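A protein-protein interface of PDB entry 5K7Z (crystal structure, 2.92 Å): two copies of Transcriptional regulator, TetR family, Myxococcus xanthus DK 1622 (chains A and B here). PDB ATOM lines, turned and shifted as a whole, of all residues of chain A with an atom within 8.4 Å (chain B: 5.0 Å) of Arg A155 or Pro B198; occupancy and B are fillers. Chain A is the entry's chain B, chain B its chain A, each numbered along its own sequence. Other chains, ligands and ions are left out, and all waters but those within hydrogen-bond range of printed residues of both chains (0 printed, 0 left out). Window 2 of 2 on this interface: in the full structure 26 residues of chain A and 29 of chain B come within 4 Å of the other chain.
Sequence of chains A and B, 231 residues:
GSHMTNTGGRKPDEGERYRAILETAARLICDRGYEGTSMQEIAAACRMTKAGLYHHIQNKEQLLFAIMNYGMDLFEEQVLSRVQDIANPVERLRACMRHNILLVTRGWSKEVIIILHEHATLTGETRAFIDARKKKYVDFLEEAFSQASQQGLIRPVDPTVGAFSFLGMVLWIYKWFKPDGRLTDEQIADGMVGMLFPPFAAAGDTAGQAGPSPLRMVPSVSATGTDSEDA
Arg A155 touches Gly B194. CB of Pro B198 touches NE of Arg A155, at 3.7 Å. Met B195 touches Val A157 (SD to CG2, 3.8 Å). CD1 of Leu A196 touches CG of Met B195 (3.4 Å).
Arg A155 touches two residues of chain B. Pro B198 touches one residue of chain A. Of the printed residues of chain B, Leu A196 touches Met B195 (3.4 Å). Of the printed residues of chain A, Met B195 touches Val A157 (3.8 Å) and Leu A196 (3.4 Å). Of the printed residues of chain A, Gly B194 touches Arg A155. Printed residues of chain B within 4 Å of Val A157: Met B195 (3.8 Å). Pro A199 touches none of the printed residues of chain B. Phe A197 touches none of the printed residues of chain B. The nearest residue of chain A that does not touch Pro B198 is Met A195 (7.0 Å).
Hydrophobic or aromatic side chains of chain B that line the printed part of chain A: Met B195 and Pro B198. Along chain B the printed residues that touch a printed residue of chain A span positions 194 to 198. Of the 18 printed residues of chain A, 3 touch a printed residue of chain B.
Leu A196 touches Met B195, but with the chains exchanged Met A195 does not touch Leu B196 (4.1 Å).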
ATOM      1  N   VAL A  90      21.335 -18.737 -11.279  1.00  0.00           N
ATOM      2  CA  VAL A  90      20.866 -19.022 -12.632  1.00  0.00           C
ATOM      3  C   VAL A  90      21.784 -18.374 -13.660  1.00  0.00           C
ATOM      4  O   VAL A  90      22.065 -18.954 -14.714  1.00  0.00           O
ATOM      5  CB  VAL A  90      19.403 -18.570 -12.803  1.00  0.00           C
ATOM      6  CG1 VAL A  90      19.286 -17.049 -12.785  1.00  0.00           C
ATOM      7  CG2 VAL A  90      18.818 -19.141 -14.084  1.00  0.00           C
ATOM      8  N   PHE A 145      21.663 -25.497  -8.852  1.00  0.00           N
ATOM      9  CA  PHE A 145      20.256 -25.814  -9.073  1.00  0.00           C
ATOM     10  C   PHE A 145      19.458 -25.743  -7.779  1.00  0.00           C
ATOM     11  O   PHE A 145      18.258 -25.457  -7.810  1.00  0.00           O
ATOM     12  CB  PHE A 145      20.113 -27.201  -9.701  1.00  0.00           C
ATOM     13  CG  PHE A 145      20.168 -27.195 -11.200  1.00  0.00           C
ATOM     14  CD1 PHE A 145      19.029 -26.954 -11.943  1.00  0.00           C
ATOM     15  CD2 PHE A 145      21.358 -27.426 -11.866  1.00  0.00           C
ATOM     16  CE1 PHE A 145      19.075 -26.942 -13.317  1.00  0.00           C
ATOM     17  CE2 PHE A 145      21.407 -27.416 -13.241  1.00  0.00           C
ATOM     18  CZ  PHE A 145      20.264 -27.173 -13.967  1.00  0.00           C
ATOM     19  N   ALA A 148      19.158 -21.580  -7.136  1.00  0.00           N
ATOM     20  CA  ALA A 148      18.176 -20.984  -8.036  1.00  0.00           C
ATOM     21  C   ALA A 148      16.769 -21.475  -7.722  1.00  0.00           C
ATOM     22  O   ALA A 148      15.828 -20.680  -7.629  1.00  0.00           O
ATOM     23  CB  ALA A 148      18.542 -21.300  -9.485  1.00  0.00           C
ATOM     24  N   SER A 149      16.606 -22.787  -7.547  1.00  0.00           N
ATOM     25  CA  SER A 149      15.278 -23.340  -7.305  1.00  0.00           C
ATOM     26  C   SER A 149      14.672 -22.815  -6.012  1.00  0.00           C
ATOM     27  O   SER A 149      13.446 -22.701  -5.906  1.00  0.00           O
ATOM     28  CB  SER A 149      15.340 -24.866  -7.271  1.00  0.00           C
ATOM     29  OG  SER A 149      14.085 -25.412  -6.905  1.00  0.00           O
ATOM     30  N   GLN A 150      15.500 -22.500  -5.017  1.00  0.00           N
ATOM     31  CA  GLN A 150      14.992 -22.008  -3.741  1.00  0.00           C
ATOM     32  C   GLN A 150      14.736 -20.506  -3.759  1.00  0.00           C
ATOM     33  O   GLN A 150      13.763 -20.039  -3.160  1.00  0.00           O
ATOM     34  CB  GLN A 150      15.966 -22.355  -2.615  1.00  0.00           C
ATOM     35  CG  GLN A 150      15.973 -23.829  -2.256  1.00  0.00           C
ATOM     36  CD  GLN A 150      16.743 -24.121  -0.991  1.00  0.00           C
ATOM     37  OE1 GLN A 150      17.962 -24.283  -1.009  1.00  0.00           O
ATOM     38  NE2 GLN A 150      16.030 -24.195   0.120  1.00  0.00           N
ATOM     39  N   GLY A 152      13.582 -18.958  -6.125  1.00  0.00           N
ATOM     40  CA  GLY A 152      12.508 -18.691  -7.061  1.00  0.00           C
ATOM     41  C   GLY A 152      12.972 -18.189  -8.408  1.00  0.00           C
ATOM     42  O   GLY A 152      12.215 -17.502  -9.099  1.00  0.00           O
ATOM     43  N   LEU A 153      14.202 -18.513  -8.803  1.00  0.00           N
ATOM     44  CA  LEU A 153      14.740 -18.084 -10.086  1.00  0.00           C
ATOM     45  C   LEU A 153      14.499 -19.091 -11.201  1.00  0.00           C
ATOM     46  O   LEU A 153      14.734 -18.766 -12.369  1.00  0.00           O
ATOM     47  CB  LEU A 153      16.243 -17.817  -9.960  1.00  0.00           C
ATOM     48  CG  LEU A 153      16.603 -16.591  -9.121  1.00  0.00           C
ATOM     49  CD1 LEU A 153      18.058 -16.643  -8.698  1.00  0.00           C
ATOM     50  CD2 LEU A 153      16.320 -15.315  -9.900  1.00  0.00           C
ATOM     51  N   ILE A 154      14.043 -20.302 -10.874  1.00  0.00           N
ATOM     52  CA  ILE A 154      13.691 -21.305 -11.871  1.00  0.00           C
ATOM     53  C   ILE A 154      12.541 -22.131 -11.320  1.00  0.00           C
ATOM     54  O   ILE A 154      12.280 -22.149 -10.116  1.00  0.00           O
ATOM     55  CB  ILE A 154      14.881 -22.224 -12.243  1.00  0.00           C
ATOM     56  CG1 ILE A 154      15.449 -22.905 -10.996  1.00  0.00           C
ATOM     57  CG2 ILE A 154      15.962 -21.430 -12.962  1.00  0.00           C
ATOM     58  CD1 ILE A 154      16.429 -24.018 -11.299  1.00  0.00           C
ATOM     59  N   ARG A 155      11.842 -22.818 -12.216  1.00  0.00           N
ATOM     60  CA  ARG A 155      10.799 -23.733 -11.786  1.00  0.00           C
ATOM     61  C   ARG A 155      11.402 -24.778 -10.850  1.00  0.00           C
ATOM     62  O   ARG A 155      12.506 -25.273 -11.108  1.00  0.00           O
ATOM     63  CB  ARG A 155      10.151 -24.409 -12.995  1.00  0.00           C
ATOM     64  CG  ARG A 155       9.053 -25.398 -12.645  1.00  0.00           C
ATOM     65  CD  ARG A 155       8.302 -25.849 -13.886  1.00  0.00           C
ATOM     66  NE  ARG A 155       7.559 -24.752 -14.501  1.00  0.00           N
ATOM     67  CZ  ARG A 155       6.328 -24.385 -14.153  1.00  0.00           C
ATOM     68  NH1 ARG A 155       5.679 -25.025 -13.189  1.00  0.00           N
ATOM     69  NH2 ARG A 155       5.742 -23.371 -14.774  1.00  0.00           N
ATOM     70  N   PRO A 156      10.726 -25.130  -9.757  1.00  0.00           N
ATOM     71  CA  PRO A 156      11.310 -26.094  -8.818  1.00  0.00           C
ATOM     72  C   PRO A 156      11.759 -27.364  -9.527  1.00  0.00           C
ATOM     73  O   PRO A 156      11.097 -27.852 -10.445  1.00  0.00           O
ATOM     74  CB  PRO A 156      10.168 -26.365  -7.833  1.00  0.00           C
ATOM     75  CG  PRO A 156       9.322 -25.155  -7.896  1.00  0.00           C
ATOM     76  CD  PRO A 156       9.396 -24.678  -9.315  1.00  0.00           C
ATOM     77  N   VAL A 157      12.901 -27.896  -9.093  1.00  0.00           N
ATOM     78  CA  VAL A 157      13.463 -29.102  -9.688  1.00  0.00           C
ATOM     79  C   VAL A 157      14.444 -29.702  -8.696  1.00  0.00           C
ATOM     80  O   VAL A 157      15.115 -28.982  -7.953  1.00  0.00           O
ATOM     81  CB  VAL A 157      14.141 -28.796 -11.048  1.00  0.00           C
ATOM     82  CG1 VAL A 157      15.354 -27.895 -10.858  1.00  0.00           C
ATOM     83  CG2 VAL A 157      14.526 -30.087 -11.752  1.00  0.00           C
ATOM     84  N   ASP A 158      14.529 -31.025  -8.689  1.00  0.00           N
ATOM     85  CA  ASP A 158      15.509 -31.699  -7.852  1.00  0.00           C
ATOM     86  C   ASP A 158      16.909 -31.349  -8.344  1.00  0.00           C
ATOM     87  O   ASP A 158      17.166 -31.413  -9.551  1.00  0.00           O
ATOM     88  CB  ASP A 158      15.293 -33.207  -7.890  1.00  0.00           C
ATOM     89  CG  ASP A 158      16.145 -33.941  -6.882  1.00  0.00           C
ATOM     90  OD1 ASP A 158      17.357 -34.103  -7.133  1.00  0.00           O
ATOM     91  OD2 ASP A 158      15.601 -34.361  -5.841  1.00  0.00           O
ATOM     92  N   MET A 195      16.325 -22.850 -23.549  1.00  0.00           N
ATOM     93  CA  MET A 195      15.416 -23.984 -23.448  1.00  0.00           C
ATOM     94  C   MET A 195      15.347 -24.526 -22.027  1.00  0.00           C
ATOM     95  O   MET A 195      14.269 -24.913 -21.561  1.00  0.00           O
ATOM     96  CB  MET A 195      15.851 -25.082 -24.417  1.00  0.00           C
ATOM     97  CG  MET A 195      15.159 -26.412 -24.197  1.00  0.00           C
ATOM     98  SD  MET A 195      15.131 -27.420 -25.683  1.00  0.00           S
ATOM     99  CE  MET A 195      13.451 -27.145 -26.222  1.00  0.00           C
ATOM    100  N   LEU A 196      16.477 -24.561 -21.323  1.00  0.00           N
ATOM    101  CA  LEU A 196      16.521 -25.061 -19.956  1.00  0.00           C
ATOM    102  C   LEU A 196      16.464 -23.957 -18.913  1.00  0.00           C
ATOM    103  O   LEU A 196      15.935 -24.182 -17.819  1.00  0.00           O
ATOM    104  CB  LEU A 196      17.792 -25.890 -19.739  1.00  0.00           C
ATOM    105  CG  LEU A 196      17.943 -26.566 -18.374  1.00  0.00           C
ATOM    106  CD1 LEU A 196      16.830 -27.567 -18.137  1.00  0.00           C
ATOM    107  CD2 LEU A 196      19.295 -27.246 -18.255  1.00  0.00           C
ATOM    108  N   PHE A 197      16.992 -22.770 -19.224  1.00  0.00           N
ATOM    109  CA  PHE A 197      16.999 -21.628 -18.311  1.00  0.00           C
ATOM    110  C   PHE A 197      16.324 -20.450 -19.002  1.00  0.00           C
ATOM    111  O   PHE A 197      16.999 -19.536 -19.498  1.00  0.00           O
ATOM    112  CB  PHE A 197      18.420 -21.263 -17.884  1.00  0.00           C
ATOM    113  CG  PHE A 197      19.173 -22.396 -17.253  1.00  0.00           C
ATOM    114  CD1 PHE A 197      18.801 -22.888 -16.017  1.00  0.00           C
ATOM    115  CD2 PHE A 197      20.257 -22.966 -17.895  1.00  0.00           C
ATOM    116  CE1 PHE A 197      19.490 -23.928 -15.438  1.00  0.00           C
ATOM    117  CE2 PHE A 197      20.949 -24.006 -17.318  1.00  0.00           C
ATOM    118  CZ  PHE A 197      20.565 -24.488 -16.088  1.00  0.00           C
ATOM    119  N   PRO A 198      14.997 -20.439 -19.065  1.00  0.00           N
ATOM    120  CA  PRO A 198      14.291 -19.288 -19.621  1.00  0.00           C
ATOM    121  C   PRO A 198      13.993 -18.265 -18.542  1.00  0.00           C
ATOM    122  O   PRO A 198      14.093 -18.570 -17.344  1.00  0.00           O
ATOM    123  CB  PRO A 198      13.002 -19.908 -20.175  1.00  0.00           C
ATOM    124  CG  PRO A 198      12.733 -21.051 -19.249  1.00  0.00           C
ATOM    125  CD  PRO A 198      14.079 -21.556 -18.772  1.00  0.00           C
ATOM    126  N   PRO A 199      13.629 -17.040 -18.918  1.00  0.00           N
ATOM    127  CA  PRO A 199      13.206 -16.064 -17.908  1.00  0.00           C
ATOM    128  C   PRO A 199      11.962 -16.551 -17.177  1.00  0.00           C
ATOM    129  O   PRO A 199      11.004 -17.024 -17.792  1.00  0.00           O
ATOM    130  CB  PRO A 199      12.933 -14.796 -18.727  1.00  0.00           C
ATOM    131  CG  PRO A 199      12.736 -15.269 -20.128  1.00  0.00           C
ATOM    132  CD  PRO A 199      13.605 -16.476 -20.277  1.00  0.00           C
ATOM    133  N   PHE A 200      11.989 -16.435 -15.853  1.00  0.00           N
ATOM    134  CA  PHE A 200      10.927 -16.972 -15.010  1.00  0.00           C
ATOM    135  C   PHE A 200      10.359 -15.895 -14.091  1.00  0.00           C
ATOM    136  O   PHE A 200      10.676 -15.849 -12.902  1.00  0.00           O
ATOM    137  CB  PHE A 200      11.455 -18.150 -14.188  1.00  0.00           C
ATOM    138  CG  PHE A 200      10.401 -18.855 -13.384  1.00  0.00           C
ATOM    139  CD1 PHE A 200       9.448 -19.643 -14.007  1.00  0.00           C
ATOM    140  CD2 PHE A 200      10.373 -18.743 -12.005  1.00  0.00           C
ATOM    141  CE1 PHE A 200       8.480 -20.297 -13.268  1.00  0.00           C
ATOM    142  CE2 PHE A 200       9.408 -19.396 -11.262  1.00  0.00           C
ATOM    143  CZ  PHE A 200       8.462 -20.174 -11.893  1.00  0.00           C
ATOM    144  N   ARG B  94       6.192 -36.059 -24.167  1.00  0.00           N
ATOM    145  CA  ARG B  94       6.231 -36.424 -22.754  1.00  0.00           C
ATOM    146  C   ARG B  94       6.282 -37.935 -22.578  1.00  0.00           C
ATOM    147  O   ARG B  94       7.045 -38.442 -21.749  1.00  0.00           O
ATOM    148  CB  ARG B  94       5.021 -35.847 -22.020  1.00  0.00           C
ATOM    149  CG  ARG B  94       5.067 -34.343 -21.804  1.00  0.00           C
ATOM    150  CD  ARG B  94       4.078 -33.919 -20.730  1.00  0.00           C
ATOM    151  NE  ARG B  94       3.982 -32.465 -20.606  1.00  0.00           N
ATOM    152  CZ  ARG B  94       2.983 -31.719 -21.078  1.00  0.00           C
ATOM    153  NH1 ARG B  94       1.957 -32.271 -21.715  1.00  0.00           N
ATOM    154  NH2 ARG B  94       3.009 -30.407 -20.905  1.00  0.00           N
ATOM    155  N   VAL B 193      10.905 -34.598 -17.501  1.00  0.00           N
ATOM    156  CA  VAL B 193       9.757 -34.152 -18.287  1.00  0.00           C
ATOM    157  C   VAL B 193       9.324 -32.765 -17.831  1.00  0.00           C
ATOM    158  O   VAL B 193       9.324 -31.805 -18.610  1.00  0.00           O
ATOM    159  CB  VAL B 193       8.603 -35.164 -18.179  1.00  0.00           C
ATOM    160  CG1 VAL B 193       7.335 -34.618 -18.822  1.00  0.00           C
ATOM    161  CG2 VAL B 193       8.993 -36.481 -18.830  1.00  0.00           C
ATOM    162  N   GLY B 194       8.961 -32.641 -16.553  1.00  0.00           N
ATOM    163  CA  GLY B 194       8.493 -31.375 -16.019  1.00  0.00           C
ATOM    164  C   GLY B 194       9.464 -30.226 -16.196  1.00  0.00           C
ATOM    165  O   GLY B 194       9.062 -29.065 -16.082  1.00  0.00           O
ATOM    166  N   MET B 195      10.731 -30.518 -16.471  1.00  0.00           N
ATOM    167  CA  MET B 195      11.732 -29.470 -16.627  1.00  0.00           C
ATOM    168  C   MET B 195      11.846 -28.976 -18.060  1.00  0.00           C
ATOM    169  O   MET B 195      12.221 -27.818 -18.280  1.00  0.00           O
ATOM    170  CB  MET B 195      13.097 -29.974 -16.150  1.00  0.00           C
ATOM    171  CG  MET B 195      14.240 -29.010 -16.407  1.00  0.00           C
ATOM    172  SD  MET B 195      15.650 -29.330 -15.336  1.00  0.00           S
ATOM    173  CE  MET B 195      15.866 -31.085 -15.589  1.00  0.00           C
ATOM    174  N   LEU B 196      11.535 -29.822 -19.037  1.00  0.00           N
ATOM    175  CA  LEU B 196      11.577 -29.436 -20.441  1.00  0.00           C
ATOM    176  C   LEU B 196      10.198 -29.298 -21.066  1.00  0.00           C
ATOM    177  O   LEU B 196      10.038 -28.523 -22.010  1.00  0.00           O
ATOM    178  CB  LEU B 196      12.394 -30.455 -21.242  1.00  0.00           C
ATOM    179  CG  LEU B 196      13.079 -29.932 -22.505  1.00  0.00           C
ATOM    180  CD1 LEU B 196      14.388 -30.658 -22.727  1.00  0.00           C
ATOM    181  CD2 LEU B 196      12.188 -30.095 -23.719  1.00  0.00           C
ATOM    182  N   PHE B 197       9.199 -30.014 -20.557  1.00  0.00           N
ATOM    183  CA  PHE B 197       7.821 -29.907 -21.037  1.00  0.00           C
ATOM    184  C   PHE B 197       6.897 -29.588 -19.868  1.00  0.00           C
ATOM    185  O   PHE B 197       6.027 -30.385 -19.508  1.00  0.00           O
ATOM    186  CB  PHE B 197       7.388 -31.193 -21.737  1.00  0.00           C
ATOM    187  CG  PHE B 197       8.295 -31.610 -22.855  1.00  0.00           C
ATOM    188  CD1 PHE B 197       8.484 -30.791 -23.952  1.00  0.00           C
ATOM    189  CD2 PHE B 197       8.950 -32.825 -22.813  1.00  0.00           C
ATOM    190  CE1 PHE B 197       9.317 -31.173 -24.981  1.00  0.00           C
ATOM    191  CE2 PHE B 197       9.781 -33.210 -23.838  1.00  0.00           C
ATOM    192  CZ  PHE B 197       9.965 -32.383 -24.923  1.00  0.00           C
ATOM    193  N   PRO B 198       7.060 -28.425 -19.248  1.00  0.00           N
ATOM    194  CA  PRO B 198       6.182 -28.051 -18.144  1.00  0.00           C
ATOM    195  C   PRO B 198       4.831 -27.597 -18.663  1.00  0.00           C
ATOM    196  O   PRO B 198       4.709 -27.218 -19.837  1.00  0.00           O
ATOM    197  CB  PRO B 198       6.939 -26.899 -17.472  1.00  0.00           C
ATOM    198  CG  PRO B 198       7.682 -26.261 -18.592  1.00  0.00           C
ATOM    199  CD  PRO B 198       8.058 -27.378 -19.535  1.00  0.00           C
ATOM    200  N   PRO B 199       3.793 -27.629 -17.832  1.00  0.00           N
ATOM    201  CA  PRO B 199       2.506 -27.066 -18.252  1.00  0.00           C
ATOM    202  C   PRO B 199       2.670 -25.628 -18.721  1.00  0.00           C
ATOM    203  O   PRO B 199       3.219 -24.781 -18.012  1.00  0.00           O
ATOM    204  CB  PRO B 199       1.640 -27.166 -16.989  1.00  0.00           C
ATOM    205  CG  PRO B 199       2.589 -27.473 -15.865  1.00  0.00           C
ATOM    206  CD  PRO B 199       3.726 -28.206 -16.481  1.00  0.00           C
ATOM    207  N   PHE B 200       2.194 -25.358 -19.933  1.00  0.00           N
ATOM    208  CA  PHE B 200       2.415 -24.069 -20.578  1.00  0.00           C
ATOM    209  C   PHE B 200       1.119 -23.520 -21.169  1.00  0.00           C
ATOM    210  O   PHE B 200       0.808 -23.752 -22.336  1.00  0.00           O
ATOM    211  CB  PHE B 200       3.478 -24.210 -21.670  1.00  0.00           C
ATOM    212  CG  PHE B 200       3.833 -22.918 -22.346  1.00  0.00           C
ATOM    213  CD1 PHE B 200       4.700 -22.023 -21.747  1.00  0.00           C
ATOM    214  CD2 PHE B 200       3.309 -22.605 -23.589  1.00  0.00           C
ATOM    215  CE1 PHE B 200       5.032 -20.835 -22.370  1.00  0.00           C
ATOM    216  CE2 PHE B 200       3.637 -21.420 -24.217  1.00  0.00           C
ATOM    217  CZ  PHE B 200       4.499 -20.535 -23.607  1.00  0.00           C
